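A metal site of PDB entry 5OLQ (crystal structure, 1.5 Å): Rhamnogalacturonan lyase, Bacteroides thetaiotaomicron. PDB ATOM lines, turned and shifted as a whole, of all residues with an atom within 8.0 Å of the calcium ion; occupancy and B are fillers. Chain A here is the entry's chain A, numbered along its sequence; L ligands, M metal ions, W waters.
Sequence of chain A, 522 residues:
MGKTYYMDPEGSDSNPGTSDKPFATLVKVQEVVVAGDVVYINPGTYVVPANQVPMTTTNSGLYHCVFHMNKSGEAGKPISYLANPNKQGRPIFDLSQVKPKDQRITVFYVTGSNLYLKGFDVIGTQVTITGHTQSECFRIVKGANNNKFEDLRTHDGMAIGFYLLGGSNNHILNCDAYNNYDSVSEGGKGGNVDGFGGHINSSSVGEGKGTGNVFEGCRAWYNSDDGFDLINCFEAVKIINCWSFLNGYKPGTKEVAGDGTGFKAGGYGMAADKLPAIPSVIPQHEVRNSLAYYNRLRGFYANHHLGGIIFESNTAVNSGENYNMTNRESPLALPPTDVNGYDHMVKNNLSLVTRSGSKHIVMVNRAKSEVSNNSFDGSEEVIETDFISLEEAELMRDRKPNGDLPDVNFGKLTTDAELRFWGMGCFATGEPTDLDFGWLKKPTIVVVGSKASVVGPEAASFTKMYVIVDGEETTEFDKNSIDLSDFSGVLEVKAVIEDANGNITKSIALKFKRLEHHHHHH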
ATOM      1  N   ILE A 160       1.583  -2.391  22.253  1.00  0.00           N
ATOM      2  CA  ILE A 160       2.285  -3.065  23.321  1.00  0.00           C
ATOM      3  C   ILE A 160       1.976  -2.324  24.630  1.00  0.00           C
ATOM      4  O   ILE A 160       1.988  -1.071  24.691  1.00  0.00           O
ATOM      5  CB  ILE A 160       3.811  -3.062  23.068  1.00  0.00           C
ATOM      6  CG1 ILE A 160       4.159  -3.821  21.798  1.00  0.00           C
ATOM      7  CG2 ILE A 160       4.567  -3.607  24.280  1.00  0.00           C
ATOM      8  CD1 ILE A 160       5.502  -3.404  21.231  1.00  0.00           C
ATOM      9  N   GLY A 191      -0.545  -9.303  14.495  1.00  0.00           N
ATOM     10  CA  GLY A 191       0.844  -9.028  14.343  1.00  0.00           C
ATOM     11  C   GLY A 191       1.654  -9.368  15.551  1.00  0.00           C
ATOM     12  O   GLY A 191       1.673 -10.500  16.024  1.00  0.00           O
ATOM     13  N   ASN A 192       2.318  -8.335  16.035  1.00  0.00           N
ATOM     14  CA  ASN A 192       3.473  -8.437  16.865  1.00  0.00           C
ATOM     15  C   ASN A 192       3.232  -7.645  18.145  1.00  0.00           C
ATOM     16  O   ASN A 192       4.066  -6.860  18.519  1.00  0.00           O
ATOM     17  CB  ASN A 192       4.663  -7.817  16.107  1.00  0.00           C
ATOM     18  CG  ASN A 192       4.949  -8.513  14.799  1.00  0.00           C
ATOM     19  OD1 ASN A 192       5.134  -7.874  13.767  1.00  0.00           O
ATOM     20  ND2 ASN A 192       4.948  -9.842  14.836  1.00  0.00           N
ATOM     21  N   VAL A 193       2.070  -7.830  18.797  1.00  0.00           N
ATOM     22  CA  VAL A 193       1.753  -7.066  20.027  1.00  0.00           C
ATOM     23  C   VAL A 193       1.944  -7.915  21.277  1.00  0.00           C
ATOM     24  O   VAL A 193       1.259  -8.914  21.475  1.00  0.00           O
ATOM     25  CB  VAL A 193       0.331  -6.518  19.976  1.00  0.00           C
ATOM     26  CG1 VAL A 193       0.055  -5.617  21.160  1.00  0.00           C
ATOM     27  CG2 VAL A 193       0.114  -5.695  18.695  1.00  0.00           C
ATOM     28  N   ASP A 194       2.939  -7.563  22.075  1.00  0.00           N
ATOM     29  CA  ASP A 194       3.160  -8.176  23.372  1.00  0.00           C
ATOM     30  C   ASP A 194       2.497  -7.402  24.498  1.00  0.00           C
ATOM     31  O   ASP A 194       2.318  -6.185  24.420  1.00  0.00           O
ATOM     32  CB  ASP A 194       4.679  -8.220  23.699  1.00  0.00           C
ATOM     33  CG  ASP A 194       5.497  -9.054  22.749  1.00  0.00           C
ATOM     34  OD1 ASP A 194       4.978 -10.069  22.233  1.00  0.00           O
ATOM     35  OD2 ASP A 194       6.739  -8.755  22.600  1.00  0.00           O
ATOM     36  N   GLY A 195       2.209  -8.067  25.601  1.00  0.00           N
ATOM     37  CA  GLY A 195       1.750  -7.360  26.802  1.00  0.00           C
ATOM     38  C   GLY A 195       2.833  -6.512  27.454  1.00  0.00           C
ATOM     39  O   GLY A 195       2.667  -5.305  27.645  1.00  0.00           O
ATOM     40  N   PHE A 196       3.960  -7.160  27.756  1.00  0.00           N
ATOM     41  CA  PHE A 196       5.082  -6.574  28.469  1.00  0.00           C
ATOM     42  C   PHE A 196       6.357  -6.992  27.726  1.00  0.00           C
ATOM     43  O   PHE A 196       6.586  -8.178  27.504  1.00  0.00           O
ATOM     44  CB  PHE A 196       5.124  -7.120  29.892  1.00  0.00           C
ATOM     45  CG  PHE A 196       3.887  -6.852  30.719  1.00  0.00           C
ATOM     46  CD1 PHE A 196       2.806  -7.698  30.658  1.00  0.00           C
ATOM     47  CD2 PHE A 196       3.801  -5.727  31.507  1.00  0.00           C
ATOM     48  CE1 PHE A 196       1.668  -7.434  31.404  1.00  0.00           C
ATOM     49  CE2 PHE A 196       2.683  -5.466  32.253  1.00  0.00           C
ATOM     50  CZ  PHE A 196       1.611  -6.324  32.201  1.00  0.00           C
ATOM     51  N   GLY A 197       7.207  -6.026  27.415  1.00  0.00           N
ATOM     52  CA  GLY A 197       8.472  -6.263  26.758  1.00  0.00           C
ATOM     53  C   GLY A 197       9.631  -5.654  27.541  1.00  0.00           C
ATOM     54  O   GLY A 197       9.609  -4.456  27.911  1.00  0.00           O
ATOM     55  N   HIS A 199      13.539  -5.097  26.961  1.00  0.00           N
ATOM     56  CA  HIS A 199      14.523  -5.083  25.886  1.00  0.00           C
ATOM     57  C   HIS A 199      15.601  -4.030  26.155  1.00  0.00           C
ATOM     58  O   HIS A 199      15.883  -3.189  25.307  1.00  0.00           O
ATOM     59  CB  HIS A 199      13.845  -4.851  24.523  1.00  0.00           C
ATOM     60  CG  HIS A 199      12.571  -5.621  24.327  1.00  0.00           C
ATOM     61  ND1 HIS A 199      12.517  -6.995  24.153  1.00  0.00           N
ATOM     62  CD2 HIS A 199      11.290  -5.197  24.249  1.00  0.00           C
ATOM     63  CE1 HIS A 199      11.267  -7.364  23.949  1.00  0.00           C
ATOM     64  NE2 HIS A 199      10.501  -6.288  24.015  1.00  0.00           N
ATOM     65  N   SER A 224      -1.737 -10.339  21.023  1.00  0.00           N
ATOM     66  CA  SER A 224      -1.622 -11.100  19.766  1.00  0.00           C
ATOM     67  C   SER A 224      -0.387 -11.968  19.679  1.00  0.00           C
ATOM     68  O   SER A 224      -0.425 -13.068  19.084  1.00  0.00           O
ATOM     69  CB  SER A 224      -1.715 -10.206  18.526  1.00  0.00           C
ATOM     70  OG  SER A 224      -0.704  -9.274  18.441  1.00  0.00           O
ATOM     71  N   ASP A 225       0.704 -11.504  20.269  1.00  0.00           N
ATOM     72  CA  ASP A 225       1.989 -12.186  20.168  1.00  0.00           C
ATOM     73  C   ASP A 225       2.255 -12.898  21.501  1.00  0.00           C
ATOM     74  O   ASP A 225       1.745 -14.007  21.693  1.00  0.00           O
ATOM     75  CB  ASP A 225       3.057 -11.171  19.714  1.00  0.00           C
ATOM     76  CG  ASP A 225       4.247 -11.813  19.106  1.00  0.00           C
ATOM     77  OD1 ASP A 225       4.097 -12.842  18.424  1.00  0.00           O
ATOM     78  OD2 ASP A 225       5.367 -11.239  19.258  1.00  0.00           O
ATOM     79  N   ASP A 226       3.035 -12.322  22.389  1.00  0.00           N
ATOM     80  CA  ASP A 226       3.451 -12.974  23.633  1.00  0.00           C
ATOM     81  C   ASP A 226       2.967 -12.173  24.867  1.00  0.00           C
ATOM     82  O   ASP A 226       2.785 -10.975  24.798  1.00  0.00           O
ATOM     83  CB  ASP A 226       4.958 -13.058  23.658  1.00  0.00           C
ATOM     84  CG  ASP A 226       5.534 -13.662  22.399  1.00  0.00           C
ATOM     85  OD1 ASP A 226       5.166 -14.829  22.086  1.00  0.00           O
ATOM     86  OD2 ASP A 226       6.391 -12.981  21.748  1.00  0.00           O
ATOM     87  N   GLY A 227       2.783 -12.826  26.009  1.00  0.00           N
ATOM     88  CA  GLY A 227       2.437 -12.106  27.218  1.00  0.00           C
ATOM     89  C   GLY A 227       3.562 -11.230  27.720  1.00  0.00           C
ATOM     90  O   GLY A 227       3.401 -10.004  27.942  1.00  0.00           O
ATOM     91  N   PHE A 228       4.730 -11.860  27.863  1.00  0.00           N
ATOM     92  CA  PHE A 228       5.962 -11.254  28.324  1.00  0.00           C
ATOM     93  C   PHE A 228       7.066 -11.698  27.353  1.00  0.00           C
ATOM     94  O   PHE A 228       7.160 -12.890  27.033  1.00  0.00           O
ATOM     95  CB  PHE A 228       6.330 -11.721  29.755  1.00  0.00           C
ATOM     96  CG  PHE A 228       5.330 -11.337  30.822  1.00  0.00           C
ATOM     97  CD1 PHE A 228       4.128 -12.018  30.968  1.00  0.00           C
ATOM     98  CD2 PHE A 228       5.582 -10.258  31.644  1.00  0.00           C
ATOM     99  CE1 PHE A 228       3.205 -11.643  31.935  1.00  0.00           C
ATOM    100  CE2 PHE A 228       4.661  -9.873  32.611  1.00  0.00           C
ATOM    101  CZ  PHE A 228       3.468 -10.555  32.737  1.00  0.00           C
ATOM    102  N   ASP A 229       7.941 -10.754  26.950  1.00  0.00           N
ATOM    103  CA  ASP A 229       8.978 -10.984  25.967  1.00  0.00           C
ATOM    104  C   ASP A 229      10.233 -10.228  26.383  1.00  0.00           C
ATOM    105  O   ASP A 229      10.205  -8.979  26.464  1.00  0.00           O
ATOM    106  CB  ASP A 229       8.457 -10.524  24.579  1.00  0.00           C
ATOM    107  CG  ASP A 229       9.390 -10.813  23.425  1.00  0.00           C
ATOM    108  OD1 ASP A 229      10.604 -10.721  23.580  1.00  0.00           O
ATOM    109  OD2 ASP A 229       8.900 -11.075  22.313  1.00  0.00           O
ATOM    110  N   LEU A 230      11.333 -10.972  26.613  1.00  0.00           N
ATOM    111  CA  LEU A 230      12.624 -10.433  27.001  1.00  0.00           C
ATOM    112  C   LEU A 230      13.712 -10.588  25.930  1.00  0.00           C
ATOM    113  O   LEU A 230      14.904 -10.650  26.240  1.00  0.00           O
ATOM    114  CB  LEU A 230      13.102 -11.088  28.314  1.00  0.00           C
ATOM    115  CG  LEU A 230      12.195 -11.078  29.529  1.00  0.00           C
ATOM    116  CD1 LEU A 230      12.838 -11.706  30.749  1.00  0.00           C
ATOM    117  CD2 LEU A 230      11.744  -9.644  29.792  1.00  0.00           C
ATOM    118  N   ILE A 231      13.324 -10.639  24.663  1.00  0.00           N
ATOM    119  CA  ILE A 231      14.335 -10.711  23.595  1.00  0.00           C
ATOM    120  C   ILE A 231      15.247  -9.461  23.612  1.00  0.00           C
ATOM    121  O   ILE A 231      14.800  -8.386  23.974  1.00  0.00           O
ATOM    122  CB  ILE A 231      13.733 -10.935  22.176  1.00  0.00           C
ATOM    123  CG1 ILE A 231      14.750 -11.609  21.228  1.00  0.00           C
ATOM    124  CG2 ILE A 231      13.123  -9.634  21.637  1.00  0.00           C
ATOM    125  CD1 ILE A 231      14.198 -11.964  19.834  1.00  0.00           C
ATOM    126  N   ASP A 259       2.692 -15.325  17.934  1.00  0.00           N
ATOM    127  CA  ASP A 259       3.497 -16.472  18.355  1.00  0.00           C
ATOM    128  C   ASP A 259       2.926 -17.207  19.571  1.00  0.00           C
ATOM    129  O   ASP A 259       3.129 -18.408  19.679  1.00  0.00           O
ATOM    130  CB  ASP A 259       4.945 -16.079  18.657  1.00  0.00           C
ATOM    131  CG  ASP A 259       5.941 -17.217  18.415  1.00  0.00           C
ATOM    132  OD1 ASP A 259       5.670 -18.100  17.580  1.00  0.00           O
ATOM    133  OD2 ASP A 259       7.042 -17.192  19.060  1.00  0.00           O
ATOM    134  N   GLY A 260       2.193 -16.526  20.454  1.00  0.00           N
ATOM    135  CA  GLY A 260       1.521 -17.240  21.531  1.00  0.00           C
ATOM    136  C   GLY A 260       2.437 -17.906  22.567  1.00  0.00           C
ATOM    137  O   GLY A 260       2.264 -19.074  22.892  1.00  0.00           O
ATOM    138  N   THR A 261       3.390 -17.155  23.088  1.00  0.00           N
ATOM    139  CA  THR A 261       4.219 -17.618  24.221  1.00  0.00           C
ATOM    140  C   THR A 261       3.737 -16.939  25.501  1.00  0.00           C
ATOM    141  O   THR A 261       3.510 -15.716  25.494  1.00  0.00           O
ATOM    142  CB  THR A 261       5.687 -17.233  24.042  1.00  0.00           C
ATOM    143  OG1 THR A 261       6.129 -17.529  22.725  1.00  0.00           O
ATOM    144  CG2 THR A 261       6.566 -17.993  25.025  1.00  0.00           C
ATOM    145  N   LYS A 264       8.477 -15.397  27.092  1.00  0.00           N
ATOM    146  CA  LYS A 264       9.619 -15.555  26.189  1.00  0.00           C
ATOM    147  C   LYS A 264      10.747 -14.881  26.975  1.00  0.00           C
ATOM    148  O   LYS A 264      10.809 -13.636  27.045  1.00  0.00           O
ATOM    149  CB  LYS A 264       9.254 -14.839  24.907  1.00  0.00           C
ATOM    150  CG  LYS A 264      10.042 -15.072  23.657  1.00  0.00           C
ATOM    151  CD  LYS A 264       9.369 -14.510  22.435  1.00  0.00           C
ATOM    152  CE  LYS A 264       8.655 -15.566  21.640  1.00  0.00           C
ATOM    153  NZ  LYS A 264       8.093 -14.941  20.418  1.00  0.00           N
ATOM    154  N   ASN A 303      13.687 -19.173  24.351  1.00  0.00           N
ATOM    155  CA  ASN A 303      13.663 -18.302  23.169  1.00  0.00           C
ATOM    156  C   ASN A 303      15.040 -18.102  22.534  1.00  0.00           C
ATOM    157  O   ASN A 303      15.393 -17.002  22.134  1.00  0.00           O
ATOM    158  CB  ASN A 303      13.083 -16.920  23.502  1.00  0.00           C
ATOM    159  CG  ASN A 303      12.676 -16.148  22.262  1.00  0.00           C
ATOM    160  OD1 ASN A 303      12.126 -16.739  21.311  1.00  0.00           O
ATOM    161  ND2 ASN A 303      12.942 -14.822  22.251  1.00  0.00           N
HETATM  162  P1  LIG L   1       9.893 -12.187  19.190  1.00  0.00           P
HETATM  163  O1  LIG L   1      10.688 -12.011  20.515  1.00  0.00           O
HETATM  164  O2  LIG L   1      10.048 -13.692  18.859  1.00  0.00           O
HETATM  165  O3  LIG L   1      10.694 -11.314  18.206  1.00  0.00           O
HETATM  166  O4  LIG L   1       8.354 -11.878  19.283  1.00  0.00           O
HETATM  167 CA    CA M   1       6.958 -10.831  21.009  1.00  0.00          CA
HETATM  168  O   HOH W   1       7.418  -9.010  19.640  1.00  0.00           O
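The side-chain carboxylate of Asp 226 is in salt-bridge range of the side-chain amino group of Lys 264, at 3.4 Å.
The side-chain carboxylate (OD1) of Asp 226 is in hydrogen-bond range of the side-chain hydroxyl (OG1) of Thr 261 (2.9 Å).
O of Asp 226 lies within hydrogen-bond range of N of Gly 195, 3.1 Å away.
The side-chain carboxylate (OD1) of Asp 229 lies within hydrogen-bond range of the backbone NH (N) of Ile 231.
The backbone carbonyl oxygen of Phe 196 is in hydrogen-bond range of the backbone NH of Asp 229, at 3.0 Å.
O of Val 193 is in hydrogen-bond range of N of Asp 225.
The side-chain carboxylate (OD1) of Asp 225 sits at hydrogen-bond distance from the backbone NH (N) of Asp 259 (2.9 Å).
N of Gly 260 sits at hydrogen-bond distance from O of Asp 225 (2.8 Å).
Four residues have an atom within 4 Å of the calcium ion: Asp 194, Asp 225, Asp 226 and Asp 229.
The calcium ion is bound by water W1, the side-chain carboxylate (OD2) of Asp 226, the side-chain carboxylate (OD2) of Asp 229, the side-chain carboxylate (OD2) of Asp 225, the side-chain carboxylate (OD1) of Asp 194, an oxygen (O4) of the ligand and the side-chain carboxylate (OD2) of Asp 194.
The calcium ion has seven donor atoms within binding distance.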
